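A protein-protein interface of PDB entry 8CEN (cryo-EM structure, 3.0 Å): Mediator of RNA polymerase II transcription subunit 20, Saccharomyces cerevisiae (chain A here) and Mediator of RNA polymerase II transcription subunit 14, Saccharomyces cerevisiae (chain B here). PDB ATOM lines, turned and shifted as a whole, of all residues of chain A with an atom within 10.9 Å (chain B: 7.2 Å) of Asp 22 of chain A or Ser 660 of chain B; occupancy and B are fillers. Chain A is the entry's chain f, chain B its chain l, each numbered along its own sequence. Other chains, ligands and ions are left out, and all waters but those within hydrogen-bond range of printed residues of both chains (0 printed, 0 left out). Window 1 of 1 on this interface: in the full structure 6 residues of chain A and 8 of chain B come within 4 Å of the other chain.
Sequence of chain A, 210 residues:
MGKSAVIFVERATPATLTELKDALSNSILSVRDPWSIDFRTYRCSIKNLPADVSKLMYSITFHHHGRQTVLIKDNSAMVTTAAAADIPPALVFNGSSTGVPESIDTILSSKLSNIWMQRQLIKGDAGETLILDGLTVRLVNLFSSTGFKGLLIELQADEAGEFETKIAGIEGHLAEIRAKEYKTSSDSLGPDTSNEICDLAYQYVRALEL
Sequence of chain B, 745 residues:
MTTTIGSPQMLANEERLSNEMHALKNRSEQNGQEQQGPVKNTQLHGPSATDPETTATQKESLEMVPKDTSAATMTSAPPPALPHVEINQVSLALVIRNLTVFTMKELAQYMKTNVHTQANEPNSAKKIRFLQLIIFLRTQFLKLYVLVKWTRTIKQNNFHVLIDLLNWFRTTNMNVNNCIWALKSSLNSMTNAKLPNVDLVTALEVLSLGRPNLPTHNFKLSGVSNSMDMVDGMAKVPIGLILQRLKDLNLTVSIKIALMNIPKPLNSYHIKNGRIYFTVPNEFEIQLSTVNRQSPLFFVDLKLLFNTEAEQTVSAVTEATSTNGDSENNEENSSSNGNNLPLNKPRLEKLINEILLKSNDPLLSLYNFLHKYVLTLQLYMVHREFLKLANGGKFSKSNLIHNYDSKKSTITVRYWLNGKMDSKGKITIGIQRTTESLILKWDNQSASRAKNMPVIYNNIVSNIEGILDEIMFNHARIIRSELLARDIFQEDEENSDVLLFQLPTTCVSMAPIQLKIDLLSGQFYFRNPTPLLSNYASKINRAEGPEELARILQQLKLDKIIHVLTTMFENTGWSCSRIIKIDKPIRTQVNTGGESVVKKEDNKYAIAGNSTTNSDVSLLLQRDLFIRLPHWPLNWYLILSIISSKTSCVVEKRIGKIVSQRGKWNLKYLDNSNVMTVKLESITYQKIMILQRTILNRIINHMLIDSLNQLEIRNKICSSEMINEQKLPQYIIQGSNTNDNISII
OG of Ser 660 of chain B sits at hydrogen-bond distance from OD1 of Asp 22 of chain A (2.6 Å).
OG1 of Thr 18 of chain A sits at hydrogen-bond distance from N of Gly 663 of chain B, 3.3 Å away.
OD2 of Asp 22 of chain A sits at hydrogen-bond distance from N of Gly 663 of chain B (3.3 Å).
The backbone NH (N) of Arg 662 of chain B is in hydrogen-bond range of the side-chain carboxylate (OD2) of Asp 22 of chain A (3.1 Å).
Thr 18 of chain A touches Arg 662 of chain B.
Glu 19 of chain A touches Arg 662 of chain B.
Gln 661 of chain B touches Asp 22 of chain A.
Ser 25 of chain A touches Trp 665 of chain B.
Of the 11 printed residues of chain B, 5 touch a printed residue of chain A.
Printed residues of chain B that touch a printed residue of chain A: Ser 660, Gln 661, Arg 662, Gly 663 and Trp 665.
Hydrophobic or aromatic side chains of chain B within 4 Å of the printed part of chain A: Trp 665.
Printed residues of chain A that touch a printed residue of chain B: Thr 18, Glu 19, Asp 22 and Ser 25.
Of the printed residues of chain A, Ser 660 of chain B touches Asp 22 (2.6 Å).
Val 659 of chain B touches none of the printed residues of chain A.
Gln 661 of chain B touches just one residue of chain A: Asp 22 (3.8 Å).
Gly 663 of chain B touches two residues of chain A.
Trp 665 of chain B touches just one residue of chain A: Ser 25.
No residue of chain A comes within 4 Å of Asn 666 of chain B.
Of the printed residues of chain B, Ser 25 of chain A touches Trp 665.
Printed residues of chain B within 4 Å of Thr 18 of chain A: Arg 662 and Gly 663.
Of the printed residues of chain B, Glu 19 of chain A touches Arg 662.
Of the printed residues of chain A, Arg 662 of chain B touches Thr 18 (3.9 Å), Glu 19 (3.8 Å) and Asp 22 (3.1 Å).
Glu 176 of chain A touches none of the printed residues of chain B.
Leu 151 of chain A touches none of the printed residues of chain B.
The nearest residue of chain A that does not touch Ser 660 of chain B is Ser 25 of chain A (5.3 Å).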
ATOM      1  N   PRO A  14      -1.737  -7.834 -31.644  1.00  0.00           N
ATOM      2  CA  PRO A  14      -2.544  -8.131 -30.451  1.00  0.00           C
ATOM      3  C   PRO A  14      -2.505  -7.049 -29.379  1.00  0.00           C
ATOM      4  O   PRO A  14      -3.523  -6.816 -28.715  1.00  0.00           O
ATOM      5  CB  PRO A  14      -1.898  -9.429 -29.942  1.00  0.00           C
ATOM      6  CG  PRO A  14      -1.123 -10.000 -31.173  1.00  0.00           C
ATOM      7  CD  PRO A  14      -1.451  -9.098 -32.331  1.00  0.00           C
ATOM      8  N   ALA A  15      -1.367  -6.382 -29.193  1.00  0.00           N
ATOM      9  CA  ALA A  15      -1.211  -5.372 -28.152  1.00  0.00           C
ATOM     10  C   ALA A  15      -1.689  -3.990 -28.578  1.00  0.00           C
ATOM     11  O   ALA A  15      -1.487  -3.023 -27.831  1.00  0.00           O
ATOM     12  CB  ALA A  15       0.252  -5.295 -27.708  1.00  0.00           C
ATOM     13  N   THR A  16      -2.305  -3.872 -29.758  1.00  0.00           N
ATOM     14  CA  THR A  16      -2.781  -2.576 -30.230  1.00  0.00           C
ATOM     15  C   THR A  16      -3.891  -2.028 -29.338  1.00  0.00           C
ATOM     16  O   THR A  16      -4.050  -0.809 -29.231  1.00  0.00           O
ATOM     17  CB  THR A  16      -3.257  -2.698 -31.682  1.00  0.00           C
ATOM     18  OG1 THR A  16      -2.291  -3.444 -32.431  1.00  0.00           O
ATOM     19  CG2 THR A  16      -3.394  -1.326 -32.328  1.00  0.00           C
ATOM     20  N   LEU A  17      -4.636  -2.908 -28.662  1.00  0.00           N
ATOM     21  CA  LEU A  17      -5.661  -2.475 -27.714  1.00  0.00           C
ATOM     22  C   LEU A  17      -5.053  -1.667 -26.572  1.00  0.00           C
ATOM     23  O   LEU A  17      -5.461  -0.527 -26.311  1.00  0.00           O
ATOM     24  CB  LEU A  17      -6.416  -3.699 -27.182  1.00  0.00           C
ATOM     25  CG  LEU A  17      -7.658  -3.572 -26.288  1.00  0.00           C
ATOM     26  CD1 LEU A  17      -8.540  -4.778 -26.501  1.00  0.00           C
ATOM     27  CD2 LEU A  17      -7.308  -3.478 -24.807  1.00  0.00           C
ATOM     28  N   THR A  18      -4.059  -2.238 -25.885  1.00  0.00           N
ATOM     29  CA  THR A  18      -3.459  -1.522 -24.767  1.00  0.00           C
ATOM     30  C   THR A  18      -2.585  -0.367 -25.247  1.00  0.00           C
ATOM     31  O   THR A  18      -2.438   0.625 -24.527  1.00  0.00           O
ATOM     32  CB  THR A  18      -2.670  -2.478 -23.863  1.00  0.00           C
ATOM     33  OG1 THR A  18      -2.149  -1.754 -22.741  1.00  0.00           O
ATOM     34  CG2 THR A  18      -1.523  -3.141 -24.604  1.00  0.00           C
ATOM     35  N   GLU A  19      -2.040  -0.450 -26.468  1.00  0.00           N
ATOM     36  CA  GLU A  19      -1.306   0.691 -27.011  1.00  0.00           C
ATOM     37  C   GLU A  19      -2.232   1.874 -27.282  1.00  0.00           C
ATOM     38  O   GLU A  19      -1.895   3.020 -26.960  1.00  0.00           O
ATOM     39  CB  GLU A  19      -0.558   0.289 -28.283  1.00  0.00           C
ATOM     40  CG  GLU A  19       0.679  -0.581 -28.053  1.00  0.00           C
ATOM     41  CD  GLU A  19       1.643  -0.021 -27.013  1.00  0.00           C
ATOM     42  OE1 GLU A  19       1.852   1.212 -26.969  1.00  0.00           O
ATOM     43  OE2 GLU A  19       2.191  -0.824 -26.230  1.00  0.00           O
ATOM     44  N   LEU A  20      -3.411   1.613 -27.853  1.00  0.00           N
ATOM     45  CA  LEU A  20      -4.380   2.677 -28.090  1.00  0.00           C
ATOM     46  C   LEU A  20      -4.934   3.215 -26.777  1.00  0.00           C
ATOM     47  O   LEU A  20      -5.200   4.417 -26.657  1.00  0.00           O
ATOM     48  CB  LEU A  20      -5.507   2.166 -28.987  1.00  0.00           C
ATOM     49  CG  LEU A  20      -6.575   3.170 -29.425  1.00  0.00           C
ATOM     50  CD1 LEU A  20      -5.941   4.337 -30.164  1.00  0.00           C
ATOM     51  CD2 LEU A  20      -7.626   2.491 -30.288  1.00  0.00           C
ATOM     52  N   LYS A  21      -5.104   2.341 -25.778  1.00  0.00           N
ATOM     53  CA  LYS A  21      -5.533   2.799 -24.459  1.00  0.00           C
ATOM     54  C   LYS A  21      -4.490   3.711 -23.821  1.00  0.00           C
ATOM     55  O   LYS A  21      -4.836   4.744 -23.232  1.00  0.00           O
ATOM     56  CB  LYS A  21      -5.824   1.599 -23.559  1.00  0.00           C
ATOM     57  CG  LYS A  21      -6.250   1.965 -22.148  1.00  0.00           C
ATOM     58  CD  LYS A  21      -6.886   0.783 -21.440  1.00  0.00           C
ATOM     59  CE  LYS A  21      -5.922  -0.387 -21.349  1.00  0.00           C
ATOM     60  NZ  LYS A  21      -4.694  -0.029 -20.590  1.00  0.00           N
ATOM     61  N   ASP A  22      -3.207   3.355 -23.941  1.00  0.00           N
ATOM     62  CA  ASP A  22      -2.143   4.203 -23.414  1.00  0.00           C
ATOM     63  C   ASP A  22      -2.065   5.527 -24.165  1.00  0.00           C
ATOM     64  O   ASP A  22      -1.779   6.571 -23.567  1.00  0.00           O
ATOM     65  CB  ASP A  22      -0.803   3.473 -23.488  1.00  0.00           C
ATOM     66  CG  ASP A  22      -0.725   2.304 -22.530  1.00  0.00           C
ATOM     67  OD1 ASP A  22      -1.389   2.355 -21.474  1.00  0.00           O
ATOM     68  OD2 ASP A  22       0.007   1.337 -22.830  1.00  0.00           O
ATOM     69  N   ALA A  23      -2.307   5.500 -25.478  1.00  0.00           N
ATOM     70  CA  ALA A  23      -2.287   6.732 -26.260  1.00  0.00           C
ATOM     71  C   ALA A  23      -3.463   7.637 -25.908  1.00  0.00           C
ATOM     72  O   ALA A  23      -3.325   8.865 -25.897  1.00  0.00           O
ATOM     73  CB  ALA A  23      -2.287   6.406 -27.753  1.00  0.00           C
ATOM     74  N   LEU A  24      -4.621   7.052 -25.614  1.00  0.00           N
ATOM     75  CA  LEU A  24      -5.813   7.811 -25.258  1.00  0.00           C
ATOM     76  C   LEU A  24      -5.928   8.079 -23.764  1.00  0.00           C
ATOM     77  O   LEU A  24      -6.913   8.692 -23.341  1.00  0.00           O
ATOM     78  CB  LEU A  24      -7.070   7.073 -25.731  1.00  0.00           C
ATOM     79  CG  LEU A  24      -7.319   6.964 -27.234  1.00  0.00           C
ATOM     80  CD1 LEU A  24      -8.411   5.945 -27.516  1.00  0.00           C
ATOM     81  CD2 LEU A  24      -7.699   8.318 -27.796  1.00  0.00           C
ATOM     82  N   SER A  25      -4.945   7.645 -22.965  1.00  0.00           N
ATOM     83  CA  SER A  25      -5.035   7.741 -21.508  1.00  0.00           C
ATOM     84  C   SER A  25      -5.106   9.181 -21.011  1.00  0.00           C
ATOM     85  O   SER A  25      -5.613   9.429 -19.911  1.00  0.00           O
ATOM     86  CB  SER A  25      -3.847   7.027 -20.865  1.00  0.00           C
ATOM     87  OG  SER A  25      -3.760   7.335 -19.485  1.00  0.00           O
ATOM     88  N   ASN A  26      -4.600  10.139 -21.791  1.00  0.00           N
ATOM     89  CA  ASN A  26      -4.644  11.537 -21.380  1.00  0.00           C
ATOM     90  C   ASN A  26      -6.059  12.105 -21.372  1.00  0.00           C
ATOM     91  O   ASN A  26      -6.311  13.095 -20.676  1.00  0.00           O
ATOM     92  CB  ASN A  26      -3.761  12.383 -22.298  1.00  0.00           C
ATOM     93  CG  ASN A  26      -4.295  12.452 -23.716  1.00  0.00           C
ATOM     94  OD1 ASN A  26      -4.872  11.491 -24.223  1.00  0.00           O
ATOM     95  ND2 ASN A  26      -4.107  13.596 -24.363  1.00  0.00           N
ATOM     96  N   SER A  27      -6.982  11.509 -22.126  1.00  0.00           N
ATOM     97  CA  SER A  27      -8.343  12.018 -22.233  1.00  0.00           C
ATOM     98  C   SER A  27      -9.373  11.162 -21.508  1.00  0.00           C
ATOM     99  O   SER A  27     -10.553  11.529 -21.495  1.00  0.00           O
ATOM    100  CB  SER A  27      -8.743  12.147 -23.708  1.00  0.00           C
ATOM    101  OG  SER A  27      -7.860  13.009 -24.404  1.00  0.00           O
ATOM    102  N   ILE A  28      -8.964  10.035 -20.919  1.00  0.00           N
ATOM    103  CA  ILE A  28      -9.908   9.126 -20.275  1.00  0.00           C
ATOM    104  C   ILE A  28     -10.480   9.781 -19.026  1.00  0.00           C
ATOM    105  O   ILE A  28      -9.737  10.257 -18.158  1.00  0.00           O
ATOM    106  CB  ILE A  28      -9.223   7.797 -19.924  1.00  0.00           C
ATOM    107  CG1 ILE A  28      -8.690   7.115 -21.184  1.00  0.00           C
ATOM    108  CG2 ILE A  28     -10.190   6.886 -19.165  1.00  0.00           C
ATOM    109  CD1 ILE A  28      -8.361   5.649 -21.014  1.00  0.00           C
ATOM    110  N   GLU A 128     -13.009  -3.907 -22.874  1.00  0.00           N
ATOM    111  CA  GLU A 128     -12.961  -2.800 -21.931  1.00  0.00           C
ATOM    112  C   GLU A 128     -13.830  -1.653 -22.426  1.00  0.00           C
ATOM    113  O   GLU A 128     -13.956  -1.421 -23.630  1.00  0.00           O
ATOM    114  CB  GLU A 128     -11.526  -2.312 -21.713  1.00  0.00           C
ATOM    115  CG  GLU A 128     -10.716  -3.196 -20.781  1.00  0.00           C
ATOM    116  CD  GLU A 128      -9.861  -4.196 -21.531  1.00  0.00           C
ATOM    117  OE1 GLU A 128      -9.804  -4.109 -22.773  1.00  0.00           O
ATOM    118  OE2 GLU A 128      -9.252  -5.067 -20.878  1.00  0.00           O
ATOM    119  N   LEU A 130     -14.301   2.460 -21.894  1.00  0.00           N
ATOM    120  CA  LEU A 130     -13.617   3.656 -21.434  1.00  0.00           C
ATOM    121  C   LEU A 130     -14.516   4.854 -21.706  1.00  0.00           C
ATOM    122  O   LEU A 130     -15.055   4.993 -22.809  1.00  0.00           O
ATOM    123  CB  LEU A 130     -12.275   3.803 -22.153  1.00  0.00           C
ATOM    124  CG  LEU A 130     -11.251   2.709 -21.838  1.00  0.00           C
ATOM    125  CD1 LEU A 130     -10.013   2.854 -22.704  1.00  0.00           C
ATOM    126  CD2 LEU A 130     -10.879   2.739 -20.367  1.00  0.00           C
ATOM    127  N   LEU A 132     -14.659   8.728 -22.130  1.00  0.00           N
ATOM    128  CA  LEU A 132     -13.884   9.909 -22.467  1.00  0.00           C
ATOM    129  C   LEU A 132     -14.669  11.139 -22.013  1.00  0.00           C
ATOM    130  O   LEU A 132     -15.630  11.037 -21.245  1.00  0.00           O
ATOM    131  CB  LEU A 132     -13.607   9.931 -23.970  1.00  0.00           C
ATOM    132  CG  LEU A 132     -12.487   9.057 -24.546  1.00  0.00           C
ATOM    133  CD1 LEU A 132     -12.375   9.259 -26.052  1.00  0.00           C
ATOM    134  CD2 LEU A 132     -11.156   9.312 -23.874  1.00  0.00           C
ATOM    135  N   VAL A 137     -15.740   5.217 -25.637  1.00  0.00           N
ATOM    136  CA  VAL A 137     -15.014   4.301 -26.504  1.00  0.00           C
ATOM    137  C   VAL A 137     -15.015   2.937 -25.830  1.00  0.00           C
ATOM    138  O   VAL A 137     -15.177   2.816 -24.613  1.00  0.00           O
ATOM    139  CB  VAL A 137     -13.572   4.768 -26.816  1.00  0.00           C
ATOM    140  CG1 VAL A 137     -13.586   5.980 -27.723  1.00  0.00           C
ATOM    141  CG2 VAL A 137     -12.829   5.082 -25.537  1.00  0.00           C
ATOM    142  N   LEU A 139     -13.281  -1.100 -26.426  1.00  0.00           N
ATOM    143  CA  LEU A 139     -12.307  -1.863 -27.195  1.00  0.00           C
ATOM    144  C   LEU A 139     -12.384  -3.351 -26.877  1.00  0.00           C
ATOM    145  O   LEU A 139     -12.739  -3.749 -25.763  1.00  0.00           O
ATOM    146  CB  LEU A 139     -10.885  -1.365 -26.912  1.00  0.00           C
ATOM    147  CG  LEU A 139     -10.680   0.145 -26.795  1.00  0.00           C
ATOM    148  CD1 LEU A 139      -9.296   0.455 -26.247  1.00  0.00           C
ATOM    149  CD2 LEU A 139     -10.887   0.816 -28.138  1.00  0.00           C
ATOM    150  N   LEU A 151      -8.516  -5.345 -34.552  1.00  0.00           N
ATOM    151  CA  LEU A 151      -8.865  -4.501 -33.420  1.00  0.00           C
ATOM    152  C   LEU A 151     -10.200  -3.811 -33.668  1.00  0.00           C
ATOM    153  O   LEU A 151     -10.501  -3.402 -34.792  1.00  0.00           O
ATOM    154  CB  LEU A 151      -7.774  -3.460 -33.168  1.00  0.00           C
ATOM    155  CG  LEU A 151      -7.926  -2.644 -31.884  1.00  0.00           C
ATOM    156  CD1 LEU A 151      -7.547  -3.503 -30.700  1.00  0.00           C
ATOM    157  CD2 LEU A 151      -7.095  -1.373 -31.928  1.00  0.00           C
ATOM    158  N   HIS A 173      -5.915   9.692 -33.631  1.00  0.00           N
ATOM    159  CA  HIS A 173      -5.188   8.896 -32.644  1.00  0.00           C
ATOM    160  C   HIS A 173      -4.766   7.553 -33.230  1.00  0.00           C
ATOM    161  O   HIS A 173      -3.651   7.073 -32.979  1.00  0.00           O
ATOM    162  CB  HIS A 173      -6.039   8.699 -31.392  1.00  0.00           C
ATOM    163  CG  HIS A 173      -6.033   9.879 -30.470  1.00  0.00           C
ATOM    164  ND1 HIS A 173      -7.142  10.671 -30.266  1.00  0.00           N
ATOM    165  CD2 HIS A 173      -5.053  10.398 -29.693  1.00  0.00           C
ATOM    166  CE1 HIS A 173      -6.845  11.629 -29.406  1.00  0.00           C
ATOM    167  NE2 HIS A 173      -5.583  11.485 -29.043  1.00  0.00           N
ATOM    168  N   LEU A 174      -5.632   6.955 -34.053  1.00  0.00           N
ATOM    169  CA  LEU A 174      -5.229   5.773 -34.808  1.00  0.00           C
ATOM    170  C   LEU A 174      -4.122   6.085 -35.813  1.00  0.00           C
ATOM    171  O   LEU A 174      -3.351   5.190 -36.178  1.00  0.00           O
ATOM    172  CB  LEU A 174      -6.433   5.140 -35.510  1.00  0.00           C
ATOM    173  CG  LEU A 174      -7.222   4.060 -34.752  1.00  0.00           C
ATOM    174  CD1 LEU A 174      -6.318   2.868 -34.466  1.00  0.00           C
ATOM    175  CD2 LEU A 174      -7.861   4.557 -33.464  1.00  0.00           C
ATOM    176  N   GLU A 176      -1.544   8.449 -35.285  1.00  0.00           N
ATOM    177  CA  GLU A 176      -0.263   8.418 -34.566  1.00  0.00           C
ATOM    178  C   GLU A 176       0.001   7.120 -33.807  1.00  0.00           C
ATOM    179  O   GLU A 176       1.096   6.978 -33.253  1.00  0.00           O
ATOM    180  CB  GLU A 176      -0.001   9.574 -33.565  1.00  0.00           C
ATOM    181  CG  GLU A 176       0.207  11.013 -34.094  1.00  0.00           C
ATOM    182  CD  GLU A 176      -1.039  11.804 -34.360  1.00  0.00           C
ATOM    183  OE1 GLU A 176      -2.122  11.296 -34.073  1.00  0.00           O
ATOM    184  OE2 GLU A 176      -0.931  12.947 -34.853  1.00  0.00           O
ATOM    185  N   ILE A 177      -0.932   6.165 -33.760  1.00  0.00           N
ATOM    186  CA  ILE A 177      -0.565   4.865 -33.193  1.00  0.00           C
ATOM    187  C   ILE A 177      -0.086   3.967 -34.343  1.00  0.00           C
ATOM    188  O   ILE A 177       0.116   2.757 -34.173  1.00  0.00           O
ATOM    189  CB  ILE A 177      -1.730   4.253 -32.379  1.00  0.00           C
ATOM    190  CG1 ILE A 177      -1.244   3.168 -31.407  1.00  0.00           C
ATOM    191  CG2 ILE A 177      -2.785   3.641 -33.280  1.00  0.00           C
ATOM    192  CD1 ILE A 177      -0.351   3.686 -30.301  1.00  0.00           C
ATOM    193  N   ILE B 580      -5.823   4.725 -12.897  1.00  0.00           N
ATOM    194  CA  ILE B 580      -4.375   4.660 -12.755  1.00  0.00           C
ATOM    195  C   ILE B 580      -4.026   3.983 -11.435  1.00  0.00           C
ATOM    196  O   ILE B 580      -4.710   4.175 -10.422  1.00  0.00           O
ATOM    197  CB  ILE B 580      -3.774   6.079 -12.866  1.00  0.00           C
ATOM    198  CG1 ILE B 580      -2.243   6.046 -12.912  1.00  0.00           C
ATOM    199  CG2 ILE B 580      -4.359   7.020 -11.813  1.00  0.00           C
ATOM    200  CD1 ILE B 580      -1.626   7.362 -13.325  1.00  0.00           C
ATOM    201  N   ASN B 635      -0.004  14.417 -19.752  1.00  0.00           N
ATOM    202  CA  ASN B 635       0.827  13.439 -19.036  1.00  0.00           C
ATOM    203  C   ASN B 635       1.453  14.013 -17.767  1.00  0.00           C
ATOM    204  O   ASN B 635       2.525  13.574 -17.342  1.00  0.00           O
ATOM    205  CB  ASN B 635       1.912  12.843 -19.941  1.00  0.00           C
ATOM    206  CG  ASN B 635       1.384  12.451 -21.305  1.00  0.00           C
ATOM    207  OD1 ASN B 635       1.458  13.225 -22.259  1.00  0.00           O
ATOM    208  ND2 ASN B 635       0.844  11.242 -21.405  1.00  0.00           N
ATOM    209  N   ILE B 658       3.568  10.946 -15.349  1.00  0.00           N
ATOM    210  CA  ILE B 658       3.312   9.511 -15.413  1.00  0.00           C
ATOM    211  C   ILE B 658       2.850   9.167 -16.822  1.00  0.00           C
ATOM    212  O   ILE B 658       1.872   9.739 -17.317  1.00  0.00           O
ATOM    213  CB  ILE B 658       2.260   9.079 -14.374  1.00  0.00           C
ATOM    214  CG1 ILE B 658       2.539   9.735 -13.019  1.00  0.00           C
ATOM    215  CG2 ILE B 658       2.238   7.562 -14.245  1.00  0.00           C
ATOM    216  CD1 ILE B 658       1.648   9.244 -11.897  1.00  0.00           C
ATOM    217  N   VAL B 659       3.554   8.232 -17.463  1.00  0.00           N
ATOM    218  CA  VAL B 659       3.213   7.751 -18.794  1.00  0.00           C
ATOM    219  C   VAL B 659       3.106   6.230 -18.717  1.00  0.00           C
ATOM    220  O   VAL B 659       3.883   5.564 -18.029  1.00  0.00           O
ATOM    221  CB  VAL B 659       4.261   8.198 -19.851  1.00  0.00           C
ATOM    222  CG1 VAL B 659       3.978   7.616 -21.238  1.00  0.00           C
ATOM    223  CG2 VAL B 659       4.333   9.720 -19.924  1.00  0.00           C
ATOM    224  N   SER B 660       2.129   5.682 -19.438  1.00  0.00           N
ATOM    225  CA  SER B 660       1.824   4.259 -19.407  1.00  0.00           C
ATOM    226  C   SER B 660       2.362   3.593 -20.665  1.00  0.00           C
ATOM    227  O   SER B 660       2.104   4.060 -21.779  1.00  0.00           O
ATOM    228  CB  SER B 660       0.316   4.028 -19.295  1.00  0.00           C
ATOM    229  OG  SER B 660       0.007   2.644 -19.278  1.00  0.00           O
ATOM    230  N   GLN B 661       3.112   2.508 -20.481  1.00  0.00           N
ATOM    231  CA  GLN B 661       3.713   1.764 -21.582  1.00  0.00           C
ATOM    232  C   GLN B 661       3.338   0.297 -21.451  1.00  0.00           C
ATOM    233  O   GLN B 661       3.698  -0.346 -20.457  1.00  0.00           O
ATOM    234  CB  GLN B 661       5.236   1.929 -21.592  1.00  0.00           C
ATOM    235  CG  GLN B 661       5.707   3.365 -21.753  1.00  0.00           C
ATOM    236  CD  GLN B 661       7.198   3.521 -21.522  1.00  0.00           C
ATOM    237  OE1 GLN B 661       7.647   4.514 -20.948  1.00  0.00           O
ATOM    238  NE2 GLN B 661       7.974   2.541 -21.971  1.00  0.00           N
ATOM    239  N   ARG B 662       2.620  -0.221 -22.455  1.00  0.00           N
ATOM    240  CA  ARG B 662       2.225  -1.634 -22.549  1.00  0.00           C
ATOM    241  C   ARG B 662       1.425  -2.085 -21.326  1.00  0.00           C
ATOM    242  O   ARG B 662       1.607  -3.190 -20.811  1.00  0.00           O
ATOM    243  CB  ARG B 662       3.444  -2.535 -22.770  1.00  0.00           C
ATOM    244  CG  ARG B 662       3.170  -3.769 -23.617  1.00  0.00           C
ATOM    245  CD  ARG B 662       4.382  -4.686 -23.665  1.00  0.00           C
ATOM    246  NE  ARG B 662       5.461  -4.130 -24.473  1.00  0.00           N
ATOM    247  CZ  ARG B 662       6.681  -4.643 -24.545  1.00  0.00           C
ATOM    248  NH1 ARG B 662       7.019  -5.726 -23.864  1.00  0.00           N
ATOM    249  NH2 ARG B 662       7.588  -4.052 -25.318  1.00  0.00           N
ATOM    250  N   GLY B 663       0.530  -1.220 -20.854  1.00  0.00           N
ATOM    251  CA  GLY B 663      -0.285  -1.532 -19.698  1.00  0.00           C
ATOM    252  C   GLY B 663       0.398  -1.358 -18.361  1.00  0.00           C
ATOM    253  O   GLY B 663      -0.190  -1.711 -17.333  1.00  0.00           O
ATOM    254  N   LYS B 664       1.618  -0.827 -18.339  1.00  0.00           N
ATOM    255  CA  LYS B 664       2.360  -0.588 -17.109  1.00  0.00           C
ATOM    256  C   LYS B 664       2.597   0.905 -16.953  1.00  0.00           C
ATOM    257  O   LYS B 664       3.047   1.568 -17.894  1.00  0.00           O
ATOM    258  CB  LYS B 664       3.692  -1.344 -17.110  1.00  0.00           C
ATOM    259  CG  LYS B 664       4.465  -1.239 -15.805  1.00  0.00           C
ATOM    260  CD  LYS B 664       3.631  -1.708 -14.623  1.00  0.00           C
ATOM    261  CE  LYS B 664       4.340  -1.427 -13.307  1.00  0.00           C
ATOM    262  NZ  LYS B 664       3.539  -1.873 -12.132  1.00  0.00           N
ATOM    263  N   TRP B 665       2.305   1.426 -15.765  1.00  0.00           N
ATOM    264  CA  TRP B 665       2.439   2.849 -15.485  1.00  0.00           C
ATOM    265  C   TRP B 665       3.800   3.127 -14.863  1.00  0.00           C
ATOM    266  O   TRP B 665       4.184   2.483 -13.881  1.00  0.00           O
ATOM    267  CB  TRP B 665       1.321   3.317 -14.551  1.00  0.00           C
ATOM    268  CG  TRP B 665      -0.055   3.088 -15.100  1.00  0.00           C
ATOM    269  CD1 TRP B 665      -0.787   1.938 -15.026  1.00  0.00           C
ATOM    270  CD2 TRP B 665      -0.872   4.040 -15.791  1.00  0.00           C
ATOM    271  NE1 TRP B 665      -2.005   2.112 -15.638  1.00  0.00           N
ATOM    272  CE2 TRP B 665      -2.082   3.394 -16.114  1.00  0.00           C
ATOM    273  CE3 TRP B 665      -0.697   5.373 -16.170  1.00  0.00           C
ATOM    274  CZ2 TRP B 665      -3.111   4.036 -16.799  1.00  0.00           C
ATOM    275  CZ3 TRP B 665      -1.719   6.010 -16.850  1.00  0.00           C
ATOM    276  CH2 TRP B 665      -2.910   5.341 -17.157  1.00  0.00           C
ATOM    277  N   ASN B 666       4.525   4.084 -15.436  1.00  0.00           N
ATOM    278  CA  ASN B 666       5.842   4.471 -14.954  1.00  0.00           C
ATOM    279  C   ASN B 666       5.883   5.976 -14.736  1.00  0.00           C
ATOM    280  O   ASN B 666       5.354   6.744 -15.545  1.00  0.00           O
ATOM    281  CB  ASN B 666       6.945   4.058 -15.937  1.00  0.00           C
ATOM    282  CG  ASN B 666       6.820   2.615 -16.383  1.00  0.00           C
ATOM    283  OD1 ASN B 666       6.550   1.724 -15.577  1.00  0.00           O
ATOM    284  ND2 ASN B 666       7.017   2.376 -17.675  1.00  0.00           N
